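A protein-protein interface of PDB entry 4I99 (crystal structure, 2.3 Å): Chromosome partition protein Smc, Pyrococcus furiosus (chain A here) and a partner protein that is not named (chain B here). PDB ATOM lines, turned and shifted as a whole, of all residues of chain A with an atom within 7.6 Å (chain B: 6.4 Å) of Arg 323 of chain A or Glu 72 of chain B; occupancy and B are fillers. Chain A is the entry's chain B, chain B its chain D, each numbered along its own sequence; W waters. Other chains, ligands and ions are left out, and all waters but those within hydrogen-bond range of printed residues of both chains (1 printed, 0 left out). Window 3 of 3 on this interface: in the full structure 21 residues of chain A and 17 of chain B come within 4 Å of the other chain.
Ser 321 of chain A touches Asn 67 of chain B (CB to OD1, 2.9 Å). Met 322 of chain A touches Glu 66 of chain B. NH1 of Arg 323 of chain A touches O of Ile 73 of chain B, at 3.6 Å. CE of Lys 328 of chain A touches O of Ile 73 of chain B, at 3.2 Å. CG2 of Val 330 of chain A touches CG2 of Ile 73 of chain B, 3.6 Å away.
The side-chain amide oxygen (OD1) of Asn 67 of chain B lies within hydrogen-bond range of the backbone NH (N) of Met 322 of chain A (2.9 Å). The guanidinium group (NH1) of Arg 323 of chain A lies within salt-bridge range of the side-chain carboxylate (OE2) of Glu 66 of chain B, 3.0 Å away. The side-chain amino group (NZ) of Lys 328 of chain A is in salt-bridge range of the side-chain carboxylate (OE1) of Glu 66 of chain B (2.6 Å). The side-chain carboxylate (OE1) of Glu 72 of chain B lies within salt-bridge range of the guanidinium group (NH1) of Arg 323 of chain A, at 3.7 Å. The side-chain carboxylate (OE1) of Glu 66 of chain B lies within hydrogen-bond range of the side-chain hydroxyl (OG) of Ser 321 of chain A (2.9 Å). The side-chain hydroxyl (OG) of Ser 37 of chain A sits at hydrogen-bond distance from the side-chain amide nitrogen (ND2) of Asn 67 of chain B (3.1 Å).
Of the 14 printed residues of chain B, 4 touch a printed residue of chain A. Of the 15 printed residues of chain A, 6 touch a printed residue of chain B. Printed residues of chain A that touch a printed residue of chain B: Ser 37, Ser 321, Met 322, Arg 323, Lys 328 and Val 330. Among the printed residues, 11 pairs touch across the chains. Among the printed residues, Asp or Glu carboxylates within 4 Å of a Lys or Arg side-chain nitrogen of the other chain: Arg 323 of chain A with Glu 66 of chain B (3.0 Å), Arg 323 of chain A with Glu 72 of chain B (3.7 Å) and Lys 328 of chain A with Glu 66 of chain B (2.6 Å).
The side-chain carboxylate (OE2) of Glu 66 of chain B is in hydrogen-bond range of the backbone NH (N) of Ile 73 of chain B, at 3.0 Å. O of Ser 37 of chain A lies within hydrogen-bond range of OG of Ser 327 of chain A, 2.6 Å away. N of Glu 72 of chain B lies within hydrogen-bond range of O of Val 85 of chain B, 2.9 Å away. The backbone NH (N) of Lys 328 of chain A is in hydrogen-bond range of the backbone carbonyl oxygen (O) of Ser 321 of chain A.
Water W1 lies within hydrogen-bond range of the side-chain amide oxygen of Asn 67 of chain B and the side-chain hydroxyl of Ser 37 of chain A.
Arg 323 of chain A touches just these residues of chain B: Glu 66 (3.0 Å), Glu 72 (3.1 Å) and Ile 73 (3.6 Å). Of the printed residues of chain B, Val 330 of chain A touches Ile 73 (3.6 Å). Printed residues of chain A within 4 Å of Glu 66 of chain B: Ser 321 (2.9 Å), Met 322 (3.6 Å), Arg 323 (3.0 Å) and Lys 328 (2.6 Å). Printed residues of chain B within 4 Å of Ser 321 of chain A: Glu 66 and Asn 67. The nearest residue of chain B that does not touch Arg 323 of chain A is Ile 74 of chain B (4.8 Å).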
ATOM      1  N   SER A  14       8.995  21.469 -37.152  1.00  0.00           N
ATOM      2  CA  SER A  14       8.332  21.166 -35.884  1.00  0.00           C
ATOM      3  C   SER A  14       7.738  22.349 -35.129  1.00  0.00           C
ATOM      4  O   SER A  14       7.288  22.191 -33.994  1.00  0.00           O
ATOM      5  CB  SER A  14       9.306  20.434 -34.963  1.00  0.00           C
ATOM      6  OG  SER A  14      10.284  21.338 -34.473  1.00  0.00           O
ATOM      7  N   SER A  37      13.852  18.593 -29.176  1.00  0.00           N
ATOM      8  CA  SER A  37      13.026  19.774 -28.954  1.00  0.00           C
ATOM      9  C   SER A  37      12.816  20.628 -30.190  1.00  0.00           C
ATOM     10  O   SER A  37      11.833  21.360 -30.287  1.00  0.00           O
ATOM     11  CB  SER A  37      13.644  20.640 -27.853  1.00  0.00           C
ATOM     12  OG  SER A  37      13.610  19.956 -26.614  1.00  0.00           O
ATOM     13  N   SER A  71       0.112  18.020 -35.529  1.00  0.00           N
ATOM     14  CA  SER A  71       0.481  17.432 -34.251  1.00  0.00           C
ATOM     15  C   SER A  71      -0.771  17.030 -33.477  1.00  0.00           C
ATOM     16  O   SER A  71      -1.883  17.056 -34.008  1.00  0.00           O
ATOM     17  CB  SER A  71       1.299  18.428 -33.427  1.00  0.00           C
ATOM     18  OG  SER A  71       0.586  19.641 -33.239  1.00  0.00           O
ATOM     19  N   LYS A  72      -0.574  16.660 -32.218  1.00  0.00           N
ATOM     20  CA  LYS A  72      -1.667  16.241 -31.348  1.00  0.00           C
ATOM     21  C   LYS A  72      -2.827  17.226 -31.396  1.00  0.00           C
ATOM     22  O   LYS A  72      -3.985  16.841 -31.591  1.00  0.00           O
ATOM     23  CB  LYS A  72      -1.163  16.137 -29.907  1.00  0.00           C
ATOM     24  CG  LYS A  72      -2.193  15.628 -28.912  1.00  0.00           C
ATOM     25  CD  LYS A  72      -1.649  15.710 -27.487  1.00  0.00           C
ATOM     26  CE  LYS A  72      -2.627  15.131 -26.475  1.00  0.00           C
ATOM     27  NZ  LYS A  72      -2.133  15.289 -25.081  1.00  0.00           N
ATOM     28  N   ASN A  73      -2.497  18.503 -31.236  1.00  0.00           N
ATOM     29  CA  ASN A  73      -3.500  19.554 -31.207  1.00  0.00           C
ATOM     30  C   ASN A  73      -3.544  20.481 -32.410  1.00  0.00           C
ATOM     31  O   ASN A  73      -4.143  21.556 -32.330  1.00  0.00           O
ATOM     32  CB  ASN A  73      -3.295  20.399 -29.954  1.00  0.00           C
ATOM     33  CG  ASN A  73      -3.305  19.569 -28.689  1.00  0.00           C
ATOM     34  OD1 ASN A  73      -4.050  18.595 -28.588  1.00  0.00           O
ATOM     35  ND2 ASN A  73      -2.491  19.956 -27.714  1.00  0.00           N
ATOM     36  N   GLU A  74      -2.940  20.074 -33.522  1.00  0.00           N
ATOM     37  CA  GLU A  74      -2.920  20.933 -34.702  1.00  0.00           C
ATOM     38  C   GLU A  74      -3.028  20.220 -36.041  1.00  0.00           C
ATOM     39  O   GLU A  74      -2.585  19.087 -36.204  1.00  0.00           O
ATOM     40  CB  GLU A  74      -1.635  21.792 -34.710  1.00  0.00           C
ATOM     41  CG  GLU A  74      -1.496  22.782 -33.552  1.00  0.00           C
ATOM     42  CD  GLU A  74      -0.420  23.840 -33.799  1.00  0.00           C
ATOM     43  OE1 GLU A  74      -0.339  24.361 -34.938  1.00  0.00           O
ATOM     44  OE2 GLU A  74       0.340  24.172 -32.857  1.00  0.00           O
ATOM     45  N   SER A 321      11.764  24.090 -26.200  1.00  0.00           N
ATOM     46  CA  SER A 321      11.096  22.962 -25.574  1.00  0.00           C
ATOM     47  C   SER A 321       9.944  22.538 -26.451  1.00  0.00           C
ATOM     48  O   SER A 321       9.477  23.293 -27.295  1.00  0.00           O
ATOM     49  CB  SER A 321      10.584  23.323 -24.178  1.00  0.00           C
ATOM     50  OG  SER A 321       9.632  24.359 -24.247  1.00  0.00           O
ATOM     51  N   MET A 322       9.501  21.309 -26.261  1.00  0.00           N
ATOM     52  CA  MET A 322       8.403  20.796 -27.039  1.00  0.00           C
ATOM     53  C   MET A 322       7.196  20.662 -26.131  1.00  0.00           C
ATOM     54  O   MET A 322       7.293  20.138 -25.020  1.00  0.00           O
ATOM     55  CB  MET A 322       8.778  19.446 -27.637  1.00  0.00           C
ATOM     56  CG  MET A 322       7.727  18.892 -28.545  1.00  0.00           C
ATOM     57  SD  MET A 322       8.510  18.027 -30.066  1.00  0.00           S
ATOM     58  CE  MET A 322       9.152  19.609 -30.972  1.00  0.00           C
ATOM     59  N   ARG A 323       6.060  21.156 -26.607  1.00  0.00           N
ATOM     60  CA  ARG A 323       4.823  21.098 -25.844  1.00  0.00           C
ATOM     61  C   ARG A 323       3.737  20.551 -26.764  1.00  0.00           C
ATOM     62  O   ARG A 323       3.188  21.278 -27.597  1.00  0.00           O
ATOM     63  CB  ARG A 323       4.458  22.501 -25.337  1.00  0.00           C
ATOM     64  CG  ARG A 323       3.460  22.518 -24.178  1.00  0.00           C
ATOM     65  CD  ARG A 323       3.389  23.899 -23.505  1.00  0.00           C
ATOM     66  NE  ARG A 323       2.779  24.919 -24.360  1.00  0.00           N
ATOM     67  CZ  ARG A 323       2.819  26.229 -24.119  1.00  0.00           C
ATOM     68  NH1 ARG A 323       3.445  26.696 -23.045  1.00  0.00           N
ATOM     69  NH2 ARG A 323       2.238  27.077 -24.961  1.00  0.00           N
ATOM     70  N   ASP A 324       3.463  19.256 -26.619  1.00  0.00           N
ATOM     71  CA  ASP A 324       2.450  18.557 -27.408  1.00  0.00           C
ATOM     72  C   ASP A 324       2.898  18.237 -28.826  1.00  0.00           C
ATOM     73  O   ASP A 324       2.083  18.222 -29.757  1.00  0.00           O
ATOM     74  CB  ASP A 324       1.148  19.364 -27.463  1.00  0.00           C
ATOM     75  CG  ASP A 324       0.371  19.315 -26.159  1.00  0.00           C
ATOM     76  OD1 ASP A 324       0.131  18.191 -25.657  1.00  0.00           O
ATOM     77  OD2 ASP A 324      -0.005  20.397 -25.649  1.00  0.00           O
ATOM     78  N   GLY A 325       4.191  17.973 -28.990  1.00  0.00           N
ATOM     79  CA  GLY A 325       4.712  17.650 -30.307  1.00  0.00           C
ATOM     80  C   GLY A 325       4.999  18.884 -31.135  1.00  0.00           C
ATOM     81  O   GLY A 325       5.270  18.790 -32.327  1.00  0.00           O
ATOM     82  N   VAL A 326       4.935  20.050 -30.501  1.00  0.00           N
ATOM     83  CA  VAL A 326       5.180  21.317 -31.184  1.00  0.00           C
ATOM     84  C   VAL A 326       6.277  22.088 -30.465  1.00  0.00           C
ATOM     85  O   VAL A 326       6.191  22.305 -29.260  1.00  0.00           O
ATOM     86  CB  VAL A 326       3.890  22.176 -31.223  1.00  0.00           C
ATOM     87  CG1 VAL A 326       4.203  23.575 -31.705  1.00  0.00           C
ATOM     88  CG2 VAL A 326       2.852  21.515 -32.129  1.00  0.00           C
ATOM     89  N   SER A 327       7.306  22.498 -31.201  1.00  0.00           N
ATOM     90  CA  SER A 327       8.417  23.245 -30.616  1.00  0.00           C
ATOM     91  C   SER A 327       7.988  24.629 -30.159  1.00  0.00           C
ATOM     92  O   SER A 327       7.185  25.287 -30.818  1.00  0.00           O
ATOM     93  CB  SER A 327       9.562  23.393 -31.621  1.00  0.00           C
ATOM     94  OG  SER A 327      10.077  22.133 -31.990  1.00  0.00           O
ATOM     95  N   LYS A 328       8.559  25.063 -29.042  1.00  0.00           N
ATOM     96  CA  LYS A 328       8.272  26.353 -28.436  1.00  0.00           C
ATOM     97  C   LYS A 328       9.608  26.984 -28.005  1.00  0.00           C
ATOM     98  O   LYS A 328      10.574  26.270 -27.733  1.00  0.00           O
ATOM     99  CB  LYS A 328       7.354  26.128 -27.236  1.00  0.00           C
ATOM    100  CG  LYS A 328       7.219  27.303 -26.305  1.00  0.00           C
ATOM    101  CD  LYS A 328       6.348  26.925 -25.112  1.00  0.00           C
ATOM    102  CE  LYS A 328       6.552  27.890 -23.968  1.00  0.00           C
ATOM    103  NZ  LYS A 328       7.955  27.812 -23.466  1.00  0.00           N
ATOM    104  N   VAL A 330      11.735  30.292 -25.677  1.00  0.00           N
ATOM    105  CA  VAL A 330      11.721  31.285 -24.609  1.00  0.00           C
ATOM    106  C   VAL A 330      13.075  31.981 -24.637  1.00  0.00           C
ATOM    107  O   VAL A 330      14.111  31.333 -24.542  1.00  0.00           O
ATOM    108  CB  VAL A 330      11.526  30.649 -23.213  1.00  0.00           C
ATOM    109  CG1 VAL A 330      11.497  31.731 -22.160  1.00  0.00           C
ATOM    110  CG2 VAL A 330      10.239  29.852 -23.168  1.00  0.00           C
ATOM    111  N   LEU B  65      11.301  20.443 -17.833  1.00  0.00           N
ATOM    112  CA  LEU B  65       9.995  20.211 -17.228  1.00  0.00           C
ATOM    113  C   LEU B  65       8.874  20.382 -18.245  1.00  0.00           C
ATOM    114  O   LEU B  65       7.961  19.556 -18.321  1.00  0.00           O
ATOM    115  CB  LEU B  65       9.773  21.162 -16.048  1.00  0.00           C
ATOM    116  CG  LEU B  65      10.591  20.849 -14.794  1.00  0.00           C
ATOM    117  CD1 LEU B  65      10.314  21.905 -13.744  1.00  0.00           C
ATOM    118  CD2 LEU B  65      10.235  19.458 -14.276  1.00  0.00           C
ATOM    119  N   GLU B  66       8.942  21.454 -19.026  1.00  0.00           N
ATOM    120  CA  GLU B  66       7.917  21.695 -20.030  1.00  0.00           C
ATOM    121  C   GLU B  66       7.844  20.537 -21.020  1.00  0.00           C
ATOM    122  O   GLU B  66       6.757  20.158 -21.458  1.00  0.00           O
ATOM    123  CB  GLU B  66       8.179  23.010 -20.770  1.00  0.00           C
ATOM    124  CG  GLU B  66       7.134  23.294 -21.830  1.00  0.00           C
ATOM    125  CD  GLU B  66       6.883  24.766 -22.022  1.00  0.00           C
ATOM    126  OE1 GLU B  66       7.847  25.502 -22.311  1.00  0.00           O
ATOM    127  OE2 GLU B  66       5.719  25.189 -21.888  1.00  0.00           O
ATOM    128  N   ASN B  67       9.003  19.979 -21.368  1.00  0.00           N
ATOM    129  CA  ASN B  67       9.072  18.850 -22.293  1.00  0.00           C
ATOM    130  C   ASN B  67       8.368  17.631 -21.722  1.00  0.00           C
ATOM    131  O   ASN B  67       7.653  16.931 -22.438  1.00  0.00           O
ATOM    132  CB  ASN B  67      10.528  18.489 -22.598  1.00  0.00           C
ATOM    133  CG  ASN B  67      11.055  19.189 -23.825  1.00  0.00           C
ATOM    134  OD1 ASN B  67      10.977  20.413 -23.936  1.00  0.00           O
ATOM    135  ND2 ASN B  67      11.600  18.416 -24.759  1.00  0.00           N
ATOM    136  N   GLY B  69       6.031  17.689 -19.496  1.00  0.00           N
ATOM    137  CA  GLY B  69       4.615  17.983 -19.367  1.00  0.00           C
ATOM    138  C   GLY B  69       4.295  18.444 -17.955  1.00  0.00           C
ATOM    139  O   GLY B  69       3.134  18.650 -17.599  1.00  0.00           O
ATOM    140  N   ARG B  70       5.344  18.609 -17.156  1.00  0.00           N
ATOM    141  CA  ARG B  70       5.213  19.041 -15.775  1.00  0.00           C
ATOM    142  C   ARG B  70       4.732  20.481 -15.670  1.00  0.00           C
ATOM    143  O   ARG B  70       3.750  20.758 -14.991  1.00  0.00           O
ATOM    144  CB  ARG B  70       6.551  18.904 -15.052  1.00  0.00           C
ATOM    145  CG  ARG B  70       7.146  17.503 -15.071  1.00  0.00           C
ATOM    146  CD  ARG B  70       6.227  16.475 -14.422  1.00  0.00           C
ATOM    147  NE  ARG B  70       6.984  15.296 -14.002  1.00  0.00           N
ATOM    148  CZ  ARG B  70       7.870  15.291 -13.005  1.00  0.00           C
ATOM    149  NH1 ARG B  70       8.107  16.401 -12.317  1.00  0.00           N
ATOM    150  NH2 ARG B  70       8.530  14.179 -12.702  1.00  0.00           N
ATOM    151  N   VAL B  71       5.426  21.401 -16.332  1.00  0.00           N
ATOM    152  CA  VAL B  71       5.028  22.803 -16.272  1.00  0.00           C
ATOM    153  C   VAL B  71       4.755  23.386 -17.645  1.00  0.00           C
ATOM    154  O   VAL B  71       4.754  22.678 -18.656  1.00  0.00           O
ATOM    155  CB  VAL B  71       6.111  23.695 -15.593  1.00  0.00           C
ATOM    156  CG1 VAL B  71       6.597  23.045 -14.303  1.00  0.00           C
ATOM    157  CG2 VAL B  71       7.260  23.953 -16.556  1.00  0.00           C
ATOM    158  N   GLU B  72       4.529  24.694 -17.654  1.00  0.00           N
ATOM    159  CA  GLU B  72       4.259  25.450 -18.866  1.00  0.00           C
ATOM    160  C   GLU B  72       4.899  26.823 -18.683  1.00  0.00           C
ATOM    161  O   GLU B  72       4.600  27.535 -17.720  1.00  0.00           O
ATOM    162  CB  GLU B  72       2.751  25.583 -19.074  1.00  0.00           C
ATOM    163  CG  GLU B  72       2.347  26.546 -20.172  1.00  0.00           C
ATOM    164  CD  GLU B  72       0.848  26.548 -20.419  1.00  0.00           C
ATOM    165  OE1 GLU B  72       0.372  27.425 -21.172  1.00  0.00           O
ATOM    166  OE2 GLU B  72       0.149  25.668 -19.862  1.00  0.00           O
ATOM    167  N   ILE B  73       5.796  27.182 -19.596  1.00  0.00           N
ATOM    168  CA  ILE B  73       6.486  28.464 -19.515  1.00  0.00           C
ATOM    169  C   ILE B  73       5.736  29.544 -20.286  1.00  0.00           C
ATOM    170  O   ILE B  73       5.259  29.314 -21.394  1.00  0.00           O
ATOM    171  CB  ILE B  73       7.930  28.334 -20.045  1.00  0.00           C
ATOM    172  CG1 ILE B  73       8.656  27.232 -19.264  1.00  0.00           C
ATOM    173  CG2 ILE B  73       8.662  29.668 -19.913  1.00  0.00           C
ATOM    174  CD1 ILE B  73      10.027  26.860 -19.808  1.00  0.00           C
ATOM    175  N   ILE B  74       5.630  30.723 -19.688  1.00  0.00           N
ATOM    176  CA  ILE B  74       4.918  31.825 -20.311  1.00  0.00           C
ATOM    177  C   ILE B  74       5.817  33.030 -20.544  1.00  0.00           C
ATOM    178  O   ILE B  74       6.537  33.462 -19.649  1.00  0.00           O
ATOM    179  CB  ILE B  74       3.727  32.292 -19.427  1.00  0.00           C
ATOM    180  CG1 ILE B  74       2.952  31.083 -18.887  1.00  0.00           C
ATOM    181  CG2 ILE B  74       2.811  33.206 -20.232  1.00  0.00           C
ATOM    182  CD1 ILE B  74       2.374  30.186 -19.952  1.00  0.00           C
ATOM    183  N   LEU B  83       7.104  33.297 -16.917  1.00  0.00           N
ATOM    184  CA  LEU B  83       6.214  32.853 -15.846  1.00  0.00           C
ATOM    185  C   LEU B  83       5.998  31.344 -15.969  1.00  0.00           C
ATOM    186  O   LEU B  83       5.880  30.814 -17.075  1.00  0.00           O
ATOM    187  CB  LEU B  83       4.871  33.593 -15.930  1.00  0.00           C
ATOM    188  CG  LEU B  83       4.922  35.123 -15.813  1.00  0.00           C
ATOM    189  CD1 LEU B  83       3.556  35.704 -16.137  1.00  0.00           C
ATOM    190  CD2 LEU B  83       5.366  35.528 -14.414  1.00  0.00           C
ATOM    191  N   VAL B  84       5.938  30.654 -14.836  1.00  0.00           N
ATOM    192  CA  VAL B  84       5.767  29.206 -14.852  1.00  0.00           C
ATOM    193  C   VAL B  84       4.480  28.727 -14.190  1.00  0.00           C
ATOM    194  O   VAL B  84       4.205  29.040 -13.033  1.00  0.00           O
ATOM    195  CB  VAL B  84       6.953  28.510 -14.152  1.00  0.00           C
ATOM    196  CG1 VAL B  84       6.909  27.008 -14.411  1.00  0.00           C
ATOM    197  CG2 VAL B  84       8.262  29.114 -14.628  1.00  0.00           C
ATOM    198  N   VAL B  85       3.697  27.954 -14.931  1.00  0.00           N
ATOM    199  CA  VAL B  85       2.452  27.412 -14.415  1.00  0.00           C
ATOM    200  C   VAL B  85       2.551  25.893 -14.438  1.00  0.00           C
ATOM    201  O   VAL B  85       2.734  25.293 -15.493  1.00  0.00           O
ATOM    202  CB  VAL B  85       1.250  27.863 -15.270  1.00  0.00           C
ATOM    203  CG1 VAL B  85      -0.001  27.099 -14.862  1.00  0.00           C
ATOM    204  CG2 VAL B  85       1.031  29.354 -15.100  1.00  0.00           C
ATOM    205  N   PRO B  86       2.449  25.254 -13.264  1.00  0.00           N
ATOM    206  CA  PRO B  86       2.530  23.793 -13.179  1.00  0.00           C
ATOM    207  C   PRO B  86       1.285  23.136 -13.761  1.00  0.00           C
ATOM    208  O   PRO B  86       0.322  23.820 -14.115  1.00  0.00           O
ATOM    209  CB  PRO B  86       2.673  23.548 -11.682  1.00  0.00           C
ATOM    210  CG  PRO B  86       1.832  24.639 -11.105  1.00  0.00           C
ATOM    211  CD  PRO B  86       2.240  25.844 -11.931  1.00  0.00           C
ATOM    212  N   MET B  87       1.312  21.810 -13.856  1.00  0.00           N
ATOM    213  CA  MET B  87       0.193  21.046 -14.401  1.00  0.00           C
ATOM    214  C   MET B  87       0.136  19.664 -13.757  1.00  0.00           C
ATOM    215  O   MET B  87       0.316  18.665 -14.489  1.00  0.00           O
ATOM    216  CB  MET B  87       0.344  20.903 -15.916  1.00  0.00           C
ATOM    217  CG  MET B  87       0.395  22.226 -16.659  1.00  0.00           C
ATOM    218  SD  MET B  87       0.800  22.022 -18.396  1.00  0.00           S
ATOM    219  CE  MET B  87      -0.827  21.699 -19.075  1.00  0.00           C
ATOM    220  OXT MET B  87      -0.081  19.598 -12.526  1.00  0.00           O
HETATM  221  O   HOH W   1      13.760  21.504 -23.575  1.00  0.00           O
